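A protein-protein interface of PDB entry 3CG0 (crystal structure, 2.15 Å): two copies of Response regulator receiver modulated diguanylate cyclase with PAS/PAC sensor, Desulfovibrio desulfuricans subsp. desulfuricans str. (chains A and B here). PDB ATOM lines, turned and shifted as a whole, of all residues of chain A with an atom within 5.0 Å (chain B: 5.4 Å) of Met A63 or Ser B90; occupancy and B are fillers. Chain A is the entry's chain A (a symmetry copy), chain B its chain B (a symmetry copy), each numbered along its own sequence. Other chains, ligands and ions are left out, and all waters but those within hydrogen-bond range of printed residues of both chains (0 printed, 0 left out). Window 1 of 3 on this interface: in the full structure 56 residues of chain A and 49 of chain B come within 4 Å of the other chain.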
ATOM      1  N   ASP A  61       1.782 -26.615 -31.214  1.00  0.00           N
ATOM      2  CA  ASP A  61       2.087 -27.088 -29.885  1.00  0.00           C
ATOM      3  C   ASP A  61       1.647 -26.067 -28.858  1.00  0.00           C
ATOM      4  O   ASP A  61       1.884 -24.875 -29.023  1.00  0.00           O
ATOM      5  CB  ASP A  61       3.564 -27.413 -29.697  1.00  0.00           C
ATOM      6  CG  ASP A  61       3.811 -28.358 -28.506  1.00  0.00           C
ATOM      7  OD1 ASP A  61       3.506 -28.002 -27.355  1.00  0.00           O
ATOM      8  OD2 ASP A  61       4.319 -29.470 -28.717  1.00  0.00           O
ATOM      9  N   ILE A  62       1.037 -26.557 -27.783  1.00  0.00           N
ATOM     10  CA  ILE A  62       0.475 -25.690 -26.756  1.00  0.00           C
ATOM     11  C   ILE A  62       1.575 -25.063 -25.870  1.00  0.00           C
ATOM     12  O   ILE A  62       1.321 -24.111 -25.121  1.00  0.00           O
ATOM     13  CB  ILE A  62      -0.574 -26.466 -25.917  1.00  0.00           C
ATOM     14  CG1 ILE A  62      -1.654 -25.503 -25.364  1.00  0.00           C
ATOM     15  CG2 ILE A  62       0.094 -27.330 -24.841  1.00  0.00           C
ATOM     16  CD1 ILE A  62      -2.862 -26.183 -24.750  1.00  0.00           C
ATOM     17  N   MET A  63       2.788 -25.611 -25.970  1.00  0.00           N
ATOM     18  CA  MET A  63       3.961 -25.179 -25.200  1.00  0.00           C
ATOM     19  C   MET A  63       4.957 -24.557 -26.167  1.00  0.00           C
ATOM     20  O   MET A  63       5.662 -25.257 -26.898  1.00  0.00           O
ATOM     21  CB  MET A  63       4.589 -26.381 -24.468  1.00  0.00           C
ATOM     22  CG  MET A  63       5.964 -26.158 -23.786  1.00  0.00           C
ATOM     23  SD  MET A  63       5.936 -25.211 -22.242  1.00  0.00           S
ATOM     24  CE  MET A  63       6.406 -23.570 -22.826  1.00  0.00           C
ATOM     25  N   LEU A  64       5.016 -23.232 -26.172  1.00  0.00           N
ATOM     26  CA  LEU A  64       5.768 -22.543 -27.194  1.00  0.00           C
ATOM     27  C   LEU A  64       6.616 -21.402 -26.625  1.00  0.00           C
ATOM     28  O   LEU A  64       6.087 -20.451 -26.049  1.00  0.00           O
ATOM     29  CB  LEU A  64       4.788 -22.030 -28.247  1.00  0.00           C
ATOM     30  CG  LEU A  64       5.142 -22.058 -29.727  1.00  0.00           C
ATOM     31  CD1 LEU A  64       5.451 -23.480 -30.198  1.00  0.00           C
ATOM     32  CD2 LEU A  64       3.948 -21.522 -30.483  1.00  0.00           C
ATOM     33  N   CYS A  65       7.931 -21.517 -26.789  1.00  0.00           N
ATOM     34  CA  CYS A  65       8.867 -20.438 -26.481  1.00  0.00           C
ATOM     35  C   CYS A  65       8.806 -19.373 -27.578  1.00  0.00           C
ATOM     36  O   CYS A  65       8.553 -19.682 -28.747  1.00  0.00           O
ATOM     37  CB  CYS A  65      10.296 -20.975 -26.354  1.00  0.00           C
ATOM     38  SG  CYS A  65      10.512 -22.207 -25.052  1.00  0.00           S
ATOM     39  N   GLY A  70       1.720 -20.821 -27.301  1.00  0.00           N
ATOM     40  CA  GLY A  70       0.949 -21.697 -28.177  1.00  0.00           C
ATOM     41  C   GLY A  70      -0.501 -21.284 -28.398  1.00  0.00           C
ATOM     42  O   GLY A  70      -0.992 -21.327 -29.525  1.00  0.00           O
ATOM     43  N   ILE A  88      -0.997 -29.616 -30.296  1.00  0.00           N
ATOM     44  CA  ILE A  88      -0.143 -30.747 -29.916  1.00  0.00           C
ATOM     45  C   ILE A  88       0.206 -30.570 -28.446  1.00  0.00           C
ATOM     46  O   ILE A  88       0.652 -29.496 -28.045  1.00  0.00           O
ATOM     47  CB  ILE A  88       1.159 -30.806 -30.756  1.00  0.00           C
ATOM     48  CG1 ILE A  88       0.842 -30.929 -32.243  1.00  0.00           C
ATOM     49  CG2 ILE A  88       2.008 -31.981 -30.329  1.00  0.00           C
ATOM     50  CD1 ILE A  88       1.920 -30.345 -33.122  1.00  0.00           C
ATOM     51  N   SER A  90       1.726 -32.241 -24.466  1.00  0.00           N
ATOM     52  CA  SER A  90       2.749 -33.050 -23.820  1.00  0.00           C
ATOM     53  C   SER A  90       2.108 -34.208 -23.059  1.00  0.00           C
ATOM     54  O   SER A  90       0.901 -34.204 -22.786  1.00  0.00           O
ATOM     55  CB  SER A  90       3.577 -32.181 -22.871  1.00  0.00           C
ATOM     56  OG  SER A  90       4.767 -32.833 -22.462  1.00  0.00           O
ATOM     57  N   GLN A  92       3.218 -35.463 -19.965  1.00  0.00           N
ATOM     58  CA  GLN A  92       3.853 -35.537 -18.625  1.00  0.00           C
ATOM     59  C   GLN A  92       3.011 -36.098 -17.472  1.00  0.00           C
ATOM     60  O   GLN A  92       2.454 -35.362 -16.645  1.00  0.00           O
ATOM     61  CB  GLN A  92       4.614 -34.250 -18.227  1.00  0.00           C
ATOM     62  CG  GLN A  92       3.859 -32.926 -18.269  1.00  0.00           C
ATOM     63  CD  GLN A  92       4.673 -31.786 -17.663  1.00  0.00           C
ATOM     64  OE1 GLN A  92       5.907 -31.841 -17.612  1.00  0.00           O
ATOM     65  NE2 GLN A  92       3.983 -30.742 -17.211  1.00  0.00           N
ATOM     66  N   ALA A 110       9.659 -25.140 -14.482  1.00  0.00           N
ATOM     67  CA  ALA A 110       8.707 -25.134 -15.586  1.00  0.00           C
ATOM     68  C   ALA A 110       9.106 -24.144 -16.672  1.00  0.00           C
ATOM     69  O   ALA A 110       9.493 -23.013 -16.364  1.00  0.00           O
ATOM     70  CB  ALA A 110       7.315 -24.803 -15.055  1.00  0.00           C
ATOM     71  N   LYS A 111       9.016 -24.573 -17.933  1.00  0.00           N
ATOM     72  CA  LYS A 111       9.133 -23.683 -19.101  1.00  0.00           C
ATOM     73  C   LYS A 111       7.869 -22.848 -19.219  1.00  0.00           C
ATOM     74  O   LYS A 111       6.779 -23.398 -19.105  1.00  0.00           O
ATOM     75  CB  LYS A 111       9.263 -24.487 -20.392  1.00  0.00           C
ATOM     76  CG  LYS A 111      10.656 -24.986 -20.703  1.00  0.00           C
ATOM     77  CD  LYS A 111      10.579 -26.360 -21.347  1.00  0.00           C
ATOM     78  CE  LYS A 111      10.792 -26.333 -22.833  1.00  0.00           C
ATOM     79  NZ  LYS A 111      10.996 -27.729 -23.330  1.00  0.00           N
ATOM     80  N   PRO A 112       7.993 -21.530 -19.478  1.00  0.00           N
ATOM     81  CA  PRO A 112       9.213 -20.729 -19.630  1.00  0.00           C
ATOM     82  C   PRO A 112       9.836 -20.357 -18.290  1.00  0.00           C
ATOM     83  O   PRO A 112       9.123 -20.033 -17.342  1.00  0.00           O
ATOM     84  CB  PRO A 112       8.730 -19.482 -20.377  1.00  0.00           C
ATOM     85  CG  PRO A 112       7.276 -19.378 -20.086  1.00  0.00           C
ATOM     86  CD  PRO A 112       6.768 -20.727 -19.679  1.00  0.00           C
ATOM     87  N   MET B  63      11.159 -34.397 -20.652  1.00  0.00           N
ATOM     88  CA  MET B  63      10.326 -34.992 -21.692  1.00  0.00           C
ATOM     89  C   MET B  63      11.093 -35.396 -22.962  1.00  0.00           C
ATOM     90  O   MET B  63      10.477 -35.735 -23.980  1.00  0.00           O
ATOM     91  CB  MET B  63       9.162 -34.054 -22.019  1.00  0.00           C
ATOM     92  CG  MET B  63       8.163 -33.855 -20.859  1.00  0.00           C
ATOM     93  SD  MET B  63       6.979 -35.219 -20.643  1.00  0.00           S
ATOM     94  CE  MET B  63       7.840 -36.371 -19.610  1.00  0.00           C
ATOM     95  N   ILE B  88      13.878 -29.720 -16.434  1.00  0.00           N
ATOM     96  CA  ILE B  88      13.133 -28.692 -17.111  1.00  0.00           C
ATOM     97  C   ILE B  88      11.820 -29.309 -17.611  1.00  0.00           C
ATOM     98  O   ILE B  88      11.809 -30.268 -18.379  1.00  0.00           O
ATOM     99  CB  ILE B  88      13.998 -28.065 -18.222  1.00  0.00           C
ATOM    100  CG1 ILE B  88      15.142 -27.272 -17.581  1.00  0.00           C
ATOM    101  CG2 ILE B  88      13.195 -27.124 -19.080  1.00  0.00           C
ATOM    102  CD1 ILE B  88      16.186 -26.847 -18.571  1.00  0.00           C
ATOM    103  N   THR B  89      10.713 -28.789 -17.101  1.00  0.00           N
ATOM    104  CA  THR B  89       9.405 -29.362 -17.371  1.00  0.00           C
ATOM    105  C   THR B  89       8.557 -28.366 -18.165  1.00  0.00           C
ATOM    106  O   THR B  89       8.991 -27.244 -18.427  1.00  0.00           O
ATOM    107  CB  THR B  89       8.693 -29.729 -16.046  1.00  0.00           C
ATOM    108  OG1 THR B  89       8.405 -28.538 -15.312  1.00  0.00           O
ATOM    109  CG2 THR B  89       9.571 -30.615 -15.179  1.00  0.00           C
ATOM    110  N   SER B  90       7.367 -28.781 -18.585  1.00  0.00           N
ATOM    111  CA  SER B  90       6.411 -27.859 -19.186  1.00  0.00           C
ATOM    112  C   SER B  90       5.488 -27.314 -18.097  1.00  0.00           C
ATOM    113  O   SER B  90       5.284 -27.965 -17.062  1.00  0.00           O
ATOM    114  CB  SER B  90       5.611 -28.565 -20.282  1.00  0.00           C
ATOM    115  OG  SER B  90       6.480 -29.195 -21.208  1.00  0.00           O
ATOM    116  N   SER B  91       4.938 -26.120 -18.315  1.00  0.00           N
ATOM    117  CA  SER B  91       3.990 -25.541 -17.356  1.00  0.00           C
ATOM    118  C   SER B  91       2.544 -25.794 -17.789  1.00  0.00           C
ATOM    119  O   SER B  91       1.711 -24.883 -17.760  1.00  0.00           O
ATOM    120  CB  SER B  91       4.243 -24.044 -17.167  1.00  0.00           C
ATOM    121  OG  SER B  91       4.207 -23.364 -18.411  1.00  0.00           O
ATOM    122  N   GLN B  92       2.257 -27.039 -18.169  1.00  0.00           N
ATOM    123  CA  GLN B  92       0.958 -27.426 -18.716  1.00  0.00           C
ATOM    124  C   GLN B  92      -0.110 -27.619 -17.623  1.00  0.00           C
ATOM    125  O   GLN B  92      -0.520 -28.742 -17.316  1.00  0.00           O
ATOM    126  CB  GLN B  92       1.117 -28.685 -19.574  1.00  0.00           C
ATOM    127  CG  GLN B  92       0.029 -28.886 -20.615  1.00  0.00           C
ATOM    128  CD  GLN B  92       0.334 -30.042 -21.540  1.00  0.00           C
ATOM    129  OE1 GLN B  92       1.106 -29.901 -22.486  1.00  0.00           O
ATOM    130  NE2 GLN B  92      -0.274 -31.196 -21.273  1.00  0.00           N
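The side-chain amide nitrogen of Gln A92 sits at hydrogen-bond distance from the backbone carbonyl oxygen of Ser B90 (3.1 Å).
OG of Ser B91 is in hydrogen-bond range of O of Lys A111 (2.7 Å).
The backbone NH (N) of Lys A111 lies within hydrogen-bond range of the backbone carbonyl oxygen (O) of Thr B89 (2.7 Å).
The side-chain hydroxyl (OG) of Ser A90 lies within hydrogen-bond range of the side-chain sulfur (SD) of Met B63, at 3.7 Å.
N of Ser A90 sits at hydrogen-bond distance from OE1 of Gln B92, at 3.1 Å.
The side-chain carboxylate (OD1) of Asp A61 sits at hydrogen-bond distance from the backbone NH (N) of Met A63, 2.9 Å away.
The backbone NH (N) of Ile A62 is in hydrogen-bond range of the backbone carbonyl oxygen (O) of Ile A88 (3.0 Å).
OE1 of Gln B92 touches CG2 of Ile A62, at 3.6 Å.
Met A63 touches Ser B90 (SD to CB, 3.9 Å).
Gln A92 touches Met B63 (CB to SD, 3.5 Å).
OE1 of Gln A92 touches CB of Thr B89, 3.8 Å away.
CA of Ala A110 touches OG1 of Thr B89, at 3.4 Å.
CB of Ser B91 touches CB of Ala A110 (3.8 Å).
Lys A111 touches Ile B88.
Ser B91 touches Pro A112 (OG to CD, 3.9 Å).
Of the printed residues of chain B, Met A63 touches Ser B90.
Printed residues of chain A within 4 Å of Ser B90: Met A63 and Gln A92.
Printed residues of chain A within 4 Å of Ile B88: Lys A111 (3.5 Å).
Of the printed residues of chain B, Lys A111 touches Ile B88, Thr B89 and Ser B91.
Printed residues of chain B within 4 Å of Ala A110: Thr B89 and Ser B91.
Of the printed residues of chain A, Thr B89 touches Gln A92 (3.8 Å), Ala A110 (3.4 Å) and Lys A111 (2.7 Å).
Printed residues of chain B within 4 Å of Gln A92: Met B63, Thr B89 and Ser B90.
Gly A70 touches none of the printed residues of chain B.
Asp A61 touches none of the printed residues of chain B.
The nearest printed residue of chain B that does not touch Pro A112 is Thr B89 (5.9 Å).
Of the 6 printed residues of chain B, 6 touch a printed residue of chain A.
Printed residues of chain B that touch a printed residue of chain A: Met B63, Ile B88, Thr B89, Ser B90, Ser B91 and Gln B92.
Met A63 touches Ser B90, and with the chains exchanged Ser A90 touches Met B63.
Ser A90 touches Gln B92, and with the chains exchanged Gln A92 touches Ser B90.
Gln A92 touches Met B63, but with the chains exchanged Met A63 does not touch Gln B92 (5.3 Å).
Positions printed for both chains: 63, 88, 90 and 92.
Of the 13 pairs that touch across the chains among the printed residues, 4 have their exchanged pair printed and touching as well.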
